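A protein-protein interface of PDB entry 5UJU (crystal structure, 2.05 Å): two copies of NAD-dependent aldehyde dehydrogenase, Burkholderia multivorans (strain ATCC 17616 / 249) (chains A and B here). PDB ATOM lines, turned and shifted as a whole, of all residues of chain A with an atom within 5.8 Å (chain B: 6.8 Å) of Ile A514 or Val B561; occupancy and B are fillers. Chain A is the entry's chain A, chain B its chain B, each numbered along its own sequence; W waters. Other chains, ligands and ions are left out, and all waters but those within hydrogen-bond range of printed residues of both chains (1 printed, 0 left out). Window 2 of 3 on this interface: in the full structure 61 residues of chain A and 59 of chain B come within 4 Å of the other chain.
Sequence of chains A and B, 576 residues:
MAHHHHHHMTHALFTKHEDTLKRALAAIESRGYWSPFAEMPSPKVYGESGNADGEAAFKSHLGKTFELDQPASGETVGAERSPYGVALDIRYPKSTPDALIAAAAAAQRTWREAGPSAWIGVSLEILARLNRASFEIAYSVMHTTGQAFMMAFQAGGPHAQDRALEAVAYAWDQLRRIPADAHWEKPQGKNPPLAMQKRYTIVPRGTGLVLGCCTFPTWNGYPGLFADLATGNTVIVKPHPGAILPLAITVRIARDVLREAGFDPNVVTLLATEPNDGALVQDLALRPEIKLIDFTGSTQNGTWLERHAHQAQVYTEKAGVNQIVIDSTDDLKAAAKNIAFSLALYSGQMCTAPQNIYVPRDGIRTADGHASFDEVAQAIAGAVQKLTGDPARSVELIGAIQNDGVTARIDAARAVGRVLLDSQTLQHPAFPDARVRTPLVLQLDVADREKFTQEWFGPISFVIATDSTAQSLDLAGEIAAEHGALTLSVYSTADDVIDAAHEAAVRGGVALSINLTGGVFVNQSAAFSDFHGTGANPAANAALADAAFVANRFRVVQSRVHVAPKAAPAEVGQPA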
ATOM      1  N   LEU A 488      -7.773  17.987  27.193  1.00  0.00           N
ATOM      2  CA  LEU A 488      -7.008  17.527  28.345  1.00  0.00           C
ATOM      3  C   LEU A 488      -6.400  18.753  29.012  1.00  0.00           C
ATOM      4  O   LEU A 488      -5.824  19.608  28.332  1.00  0.00           O
ATOM      5  CB  LEU A 488      -5.910  16.544  27.929  1.00  0.00           C
ATOM      6  CG  LEU A 488      -4.916  16.141  29.030  1.00  0.00           C
ATOM      7  CD1 LEU A 488      -5.604  15.297  30.118  1.00  0.00           C
ATOM      8  CD2 LEU A 488      -3.733  15.409  28.399  1.00  0.00           C
ATOM      9  N   SER A 489      -6.533  18.841  30.334  1.00  0.00           N
ATOM     10  CA  SER A 489      -6.113  20.007  31.104  1.00  0.00           C
ATOM     11  C   SER A 489      -5.196  19.549  32.232  1.00  0.00           C
ATOM     12  O   SER A 489      -5.496  18.566  32.917  1.00  0.00           O
ATOM     13  CB  SER A 489      -7.343  20.744  31.666  1.00  0.00           C
ATOM     14  OG  SER A 489      -7.002  21.931  32.367  1.00  0.00           O
ATOM     15  N   VAL A 490      -4.079  20.245  32.429  1.00  0.00           N
ATOM     16  CA  VAL A 490      -3.123  19.854  33.458  1.00  0.00           C
ATOM     17  C   VAL A 490      -2.783  21.057  34.333  1.00  0.00           C
ATOM     18  O   VAL A 490      -2.600  22.175  33.838  1.00  0.00           O
ATOM     19  CB  VAL A 490      -1.845  19.228  32.852  1.00  0.00           C
ATOM     20  CG1 VAL A 490      -1.112  20.223  31.966  1.00  0.00           C
ATOM     21  CG2 VAL A 490      -0.911  18.696  33.967  1.00  0.00           C
ATOM     22  N   SER A 492       0.125  21.954  37.056  1.00  0.00           N
ATOM     23  CA  SER A 492       1.383  21.591  37.696  1.00  0.00           C
ATOM     24  C   SER A 492       2.321  22.785  37.681  1.00  0.00           C
ATOM     25  O   SER A 492       2.346  23.547  36.712  1.00  0.00           O
ATOM     26  CB  SER A 492       2.052  20.401  37.003  1.00  0.00           C
ATOM     27  OG  SER A 492       3.275  20.083  37.652  1.00  0.00           O
ATOM     28  N   ILE A 498       4.826  19.038  33.314  1.00  0.00           N
ATOM     29  CA  ILE A 498       4.309  19.649  32.088  1.00  0.00           C
ATOM     30  C   ILE A 498       4.830  18.908  30.865  1.00  0.00           C
ATOM     31  O   ILE A 498       4.091  18.673  29.898  1.00  0.00           O
ATOM     32  CB  ILE A 498       4.668  21.144  32.035  1.00  0.00           C
ATOM     33  CG1 ILE A 498       4.140  21.844  33.281  1.00  0.00           C
ATOM     34  CG2 ILE A 498       4.065  21.777  30.800  1.00  0.00           C
ATOM     35  CD1 ILE A 498       2.636  21.771  33.401  1.00  0.00           C
ATOM     36  N   HIS A 502       2.587  16.925  27.917  1.00  0.00           N
ATOM     37  CA  HIS A 502       2.700  16.990  26.463  1.00  0.00           C
ATOM     38  C   HIS A 502       2.768  15.587  25.865  1.00  0.00           C
ATOM     39  O   HIS A 502       2.139  15.308  24.836  1.00  0.00           O
ATOM     40  CB  HIS A 502       3.927  17.822  26.059  1.00  0.00           C
ATOM     41  CG  HIS A 502       3.721  19.310  26.145  1.00  0.00           C
ATOM     42  ND1 HIS A 502       4.138  20.063  27.225  1.00  0.00           N
ATOM     43  CD2 HIS A 502       3.162  20.185  25.276  1.00  0.00           C
ATOM     44  CE1 HIS A 502       3.837  21.333  27.023  1.00  0.00           C
ATOM     45  NE2 HIS A 502       3.238  21.434  25.849  1.00  0.00           N
ATOM     46  N   LEU A 512      -4.063  20.074  24.595  1.00  0.00           N
ATOM     47  CA  LEU A 512      -3.642  20.260  25.982  1.00  0.00           C
ATOM     48  C   LEU A 512      -3.792  21.712  26.420  1.00  0.00           C
ATOM     49  O   LEU A 512      -3.339  22.626  25.724  1.00  0.00           O
ATOM     50  CB  LEU A 512      -2.192  19.830  26.156  1.00  0.00           C
ATOM     51  CG  LEU A 512      -1.629  19.946  27.575  1.00  0.00           C
ATOM     52  CD1 LEU A 512      -2.315  18.962  28.504  1.00  0.00           C
ATOM     53  CD2 LEU A 512      -0.127  19.726  27.566  1.00  0.00           C
ATOM     54  N   SER A 513      -4.390  21.914  27.592  1.00  0.00           N
ATOM     55  CA  SER A 513      -4.429  23.208  28.261  1.00  0.00           C
ATOM     56  C   SER A 513      -3.619  23.125  29.549  1.00  0.00           C
ATOM     57  O   SER A 513      -3.721  22.139  30.289  1.00  0.00           O
ATOM     58  CB  SER A 513      -5.878  23.626  28.553  1.00  0.00           C
ATOM     59  OG  SER A 513      -6.639  23.730  27.341  1.00  0.00           O
ATOM     60  N   ILE A 514      -2.816  24.158  29.819  1.00  0.00           N
ATOM     61  CA  ILE A 514      -1.843  24.139  30.913  1.00  0.00           C
ATOM     62  C   ILE A 514      -2.147  25.277  31.881  1.00  0.00           C
ATOM     63  O   ILE A 514      -2.200  26.444  31.473  1.00  0.00           O
ATOM     64  CB  ILE A 514      -0.405  24.257  30.386  1.00  0.00           C
ATOM     65  CG1 ILE A 514      -0.090  23.102  29.432  1.00  0.00           C
ATOM     66  CG2 ILE A 514       0.584  24.263  31.546  1.00  0.00           C
ATOM     67  CD1 ILE A 514       0.924  23.462  28.355  1.00  0.00           C
ATOM     68  N   ASN A 515      -2.338  24.933  33.157  1.00  0.00           N
ATOM     69  CA  ASN A 515      -2.452  25.900  34.262  1.00  0.00           C
ATOM     70  C   ASN A 515      -3.491  26.987  33.978  1.00  0.00           C
ATOM     71  O   ASN A 515      -3.225  28.184  34.107  1.00  0.00           O
ATOM     72  CB  ASN A 515      -1.089  26.524  34.585  1.00  0.00           C
ATOM     73  CG  ASN A 515      -0.133  25.523  35.195  1.00  0.00           C
ATOM     74  OD1 ASN A 515      -0.560  24.616  35.905  1.00  0.00           O
ATOM     75  ND2 ASN A 515       1.159  25.657  34.891  1.00  0.00           N
ATOM     76  N   LEU A 516      -4.691  26.563  33.592  1.00  0.00           N
ATOM     77  CA  LEU A 516      -5.799  27.503  33.394  1.00  0.00           C
ATOM     78  C   LEU A 516      -6.326  27.984  34.745  1.00  0.00           C
ATOM     79  O   LEU A 516      -7.166  27.331  35.369  1.00  0.00           O
ATOM     80  CB  LEU A 516      -6.906  26.854  32.573  1.00  0.00           C
ATOM     81  CG  LEU A 516      -6.572  26.396  31.153  1.00  0.00           C
ATOM     82  CD1 LEU A 516      -7.845  25.898  30.479  1.00  0.00           C
ATOM     83  CD2 LEU A 516      -5.904  27.513  30.329  1.00  0.00           C
ATOM     84  N   ALA B 195      -3.889  36.578  26.862  1.00  0.00           N
ATOM     85  CA  ALA B 195      -2.728  36.249  26.042  1.00  0.00           C
ATOM     86  C   ALA B 195      -2.259  34.836  26.355  1.00  0.00           C
ATOM     87  O   ALA B 195      -2.036  34.493  27.521  1.00  0.00           O
ATOM     88  CB  ALA B 195      -1.582  37.244  26.261  1.00  0.00           C
ATOM     89  N   MET B 196      -2.118  34.020  25.317  1.00  0.00           N
ATOM     90  CA  MET B 196      -1.675  32.645  25.461  1.00  0.00           C
ATOM     91  C   MET B 196      -0.641  32.339  24.397  1.00  0.00           C
ATOM     92  O   MET B 196      -0.686  32.885  23.290  1.00  0.00           O
ATOM     93  CB  MET B 196      -2.824  31.640  25.306  1.00  0.00           C
ATOM     94  CG  MET B 196      -4.065  31.969  26.104  1.00  0.00           C
ATOM     95  SD  MET B 196      -5.169  30.549  26.158  1.00  0.00           S
ATOM     96  CE  MET B 196      -4.393  29.547  27.430  1.00  0.00           C
ATOM     97  N   GLN B 197       0.276  31.439  24.717  1.00  0.00           N
ATOM     98  CA  GLN B 197       1.143  30.886  23.693  1.00  0.00           C
ATOM     99  C   GLN B 197       0.618  29.522  23.286  1.00  0.00           C
ATOM    100  O   GLN B 197       0.403  28.647  24.138  1.00  0.00           O
ATOM    101  CB  GLN B 197       2.599  30.764  24.143  1.00  0.00           C
ATOM    102  CG  GLN B 197       3.514  30.563  22.940  1.00  0.00           C
ATOM    103  CD  GLN B 197       4.900  30.122  23.317  1.00  0.00           C
ATOM    104  OE1 GLN B 197       5.119  29.591  24.405  1.00  0.00           O
ATOM    105  NE2 GLN B 197       5.848  30.319  22.412  1.00  0.00           N
ATOM    106  N   LYS B 198       0.408  29.354  21.988  1.00  0.00           N
ATOM    107  CA  LYS B 198       0.015  28.085  21.411  1.00  0.00           C
ATOM    108  C   LYS B 198       1.260  27.391  20.887  1.00  0.00           C
ATOM    109  O   LYS B 198       2.207  28.031  20.432  1.00  0.00           O
ATOM    110  CB  LYS B 198      -0.997  28.272  20.278  1.00  0.00           C
ATOM    111  CG  LYS B 198      -2.147  29.224  20.584  1.00  0.00           C
ATOM    112  CD  LYS B 198      -3.019  28.708  21.706  1.00  0.00           C
ATOM    113  CE  LYS B 198      -4.180  29.651  21.981  1.00  0.00           C
ATOM    114  NZ  LYS B 198      -5.235  29.638  20.915  1.00  0.00           N
ATOM    115  N   ARG B 199       1.263  26.078  20.997  1.00  0.00           N
ATOM    116  CA  ARG B 199       2.324  25.241  20.480  1.00  0.00           C
ATOM    117  C   ARG B 199       1.671  24.132  19.676  1.00  0.00           C
ATOM    118  O   ARG B 199       0.658  23.573  20.105  1.00  0.00           O
ATOM    119  CB  ARG B 199       3.178  24.671  21.633  1.00  0.00           C
ATOM    120  CG  ARG B 199       4.126  23.560  21.229  1.00  0.00           C
ATOM    121  CD  ARG B 199       4.905  23.028  22.436  1.00  0.00           C
ATOM    122  NE  ARG B 199       5.532  21.745  22.136  1.00  0.00           N
ATOM    123  CZ  ARG B 199       6.150  20.978  23.030  1.00  0.00           C
ATOM    124  NH1 ARG B 199       6.234  21.361  24.302  1.00  0.00           N
ATOM    125  NH2 ARG B 199       6.688  19.825  22.647  1.00  0.00           N
ATOM    126  N   SER B 559      -1.002  22.627  22.224  1.00  0.00           N
ATOM    127  CA  SER B 559      -1.069  22.978  23.636  1.00  0.00           C
ATOM    128  C   SER B 559      -1.169  24.493  23.775  1.00  0.00           C
ATOM    129  O   SER B 559      -0.710  25.246  22.907  1.00  0.00           O
ATOM    130  CB  SER B 559       0.155  22.457  24.401  1.00  0.00           C
ATOM    131  OG  SER B 559       1.345  23.033  23.886  1.00  0.00           O
ATOM    132  N   ARG B 560      -1.767  24.944  24.871  1.00  0.00           N
ATOM    133  CA  ARG B 560      -1.877  26.371  25.130  1.00  0.00           C
ATOM    134  C   ARG B 560      -1.566  26.647  26.586  1.00  0.00           C
ATOM    135  O   ARG B 560      -1.847  25.827  27.464  1.00  0.00           O
ATOM    136  CB  ARG B 560      -3.267  26.929  24.798  1.00  0.00           C
ATOM    137  CG  ARG B 560      -4.399  26.287  25.568  1.00  0.00           C
ATOM    138  CD  ARG B 560      -5.757  26.807  25.096  1.00  0.00           C
ATOM    139  NE  ARG B 560      -6.851  26.022  25.651  1.00  0.00           N
ATOM    140  CZ  ARG B 560      -8.139  26.306  25.482  1.00  0.00           C
ATOM    141  NH1 ARG B 560      -8.515  27.369  24.769  1.00  0.00           N
ATOM    142  NH2 ARG B 560      -9.057  25.522  26.025  1.00  0.00           N
ATOM    143  N   VAL B 561      -0.982  27.818  26.825  1.00  0.00           N
ATOM    144  CA  VAL B 561      -0.652  28.277  28.167  1.00  0.00           C
ATOM    145  C   VAL B 561      -0.688  29.801  28.145  1.00  0.00           C
ATOM    146  O   VAL B 561      -0.374  30.430  27.130  1.00  0.00           O
ATOM    147  CB  VAL B 561       0.727  27.735  28.627  1.00  0.00           C
ATOM    148  CG1 VAL B 561       1.853  28.323  27.777  1.00  0.00           C
ATOM    149  CG2 VAL B 561       0.974  27.981  30.123  1.00  0.00           C
ATOM    150  N   HIS B 562      -1.126  30.388  29.254  1.00  0.00           N
ATOM    151  CA  HIS B 562      -1.100  31.840  29.391  1.00  0.00           C
ATOM    152  C   HIS B 562       0.333  32.362  29.373  1.00  0.00           C
ATOM    153  O   HIS B 562       1.255  31.728  29.901  1.00  0.00           O
ATOM    154  CB  HIS B 562      -1.776  32.266  30.696  1.00  0.00           C
ATOM    155  CG  HIS B 562      -3.267  32.160  30.667  1.00  0.00           C
ATOM    156  ND1 HIS B 562      -4.074  33.154  30.152  1.00  0.00           N
ATOM    157  CD2 HIS B 562      -4.098  31.182  31.095  1.00  0.00           C
ATOM    158  CE1 HIS B 562      -5.339  32.788  30.260  1.00  0.00           C
ATOM    159  NE2 HIS B 562      -5.380  31.597  30.829  1.00  0.00           N
ATOM    160  N   VAL B 563       0.510  33.541  28.779  1.00  0.00           N
ATOM    161  CA  VAL B 563       1.782  34.243  28.723  1.00  0.00           C
ATOM    162  C   VAL B 563       1.506  35.730  28.921  1.00  0.00           C
ATOM    163  O   VAL B 563       0.353  36.161  29.033  1.00  0.00           O
ATOM    164  CB  VAL B 563       2.533  33.996  27.396  1.00  0.00           C
ATOM    165  CG1 VAL B 563       3.018  32.554  27.303  1.00  0.00           C
ATOM    166  CG2 VAL B 563       1.638  34.346  26.188  1.00  0.00           C
HETATM  167  O   HOH W   1      -1.398  28.951  31.857  1.00  0.00           O
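N of Arg B560 sits at hydrogen-bond distance from O of Leu A512. N of Ile A514 is in hydrogen-bond range of O of Arg B560 (3.0 Å). A ring nitrogen (NE2) of His A502 lies within hydrogen-bond range of the guanidinium group (NH1) of Arg B199 (3.4 Å). The side-chain hydroxyl of Ser A513 sits at hydrogen-bond distance from the guanidinium group of Arg B560 (2.9 Å). The side-chain hydroxyl (OG) of Ser B559 lies within hydrogen-bond range of a ring nitrogen (NE2) of His A502.
The backbone carbonyl oxygen (O) of Leu A488 is in hydrogen-bond range of the backbone NH (N) of Ser A513 (2.8 Å). The backbone NH of Gln B197 is in hydrogen-bond range of the backbone carbonyl oxygen of Val B561 (2.7 Å). O of Ile A498 is in hydrogen-bond range of ND1 of His A502 (3.0 Å). N of Val A490 lies within hydrogen-bond range of O of Ser A513 (2.9 Å). O of Arg B199 is in hydrogen-bond range of N of Ser B559 (2.9 Å).
Among the printed residues, pairs that only touch across the chains: Leu A512 with Ser B559 (3.1 Å), Ile A514 with Val B561 (3.8 Å) and Leu A516 with Met B196 (3.9 Å).
Printed residues of chain B within 4 Å of His A502: Arg B199 and Ser B559. Ile A514 touches two residues of chain B. Of the printed residues of chain B, Leu A516 touches Met B196 (3.9 Å). Of the printed residues of chain A, Ser B559 touches His A502 and Leu A512. Of the printed residues of chain A, Arg B560 touches Leu A512 (2.9 Å), Ser A513 (2.9 Å) and Ile A514 (3.0 Å). Of chain A, only Ile A514 comes within 4 Å of Val B561. The nearest residue of chain A that does not touch Val B561 is Asn A515 (5.1 Å).
Printed residues of chain B that touch a printed residue of chain A: Met B196, Arg B199, Ser B559, Arg B560 and Val B561. Hydrophobic or aromatic side chains of chain B that line the printed part of chain A: Met B196 and Val B561. Of the 11 printed residues of chain A, 5 touch a printed residue of chain B. Among the printed residues, 8 pairs touch across the chains. Among the printed residues, no Asp or Glu carboxylate lies within 4 Å of a Lys or Arg side-chain nitrogen of the other chain.
No position is printed for both chains. Of the 8 pairs that touch across the chains among the printed residues, none has its exchanged pair printed and touching as well.
Water W1 lies within hydrogen-bond range of O of Ile A514, N of His B562 and O of Asn A515.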
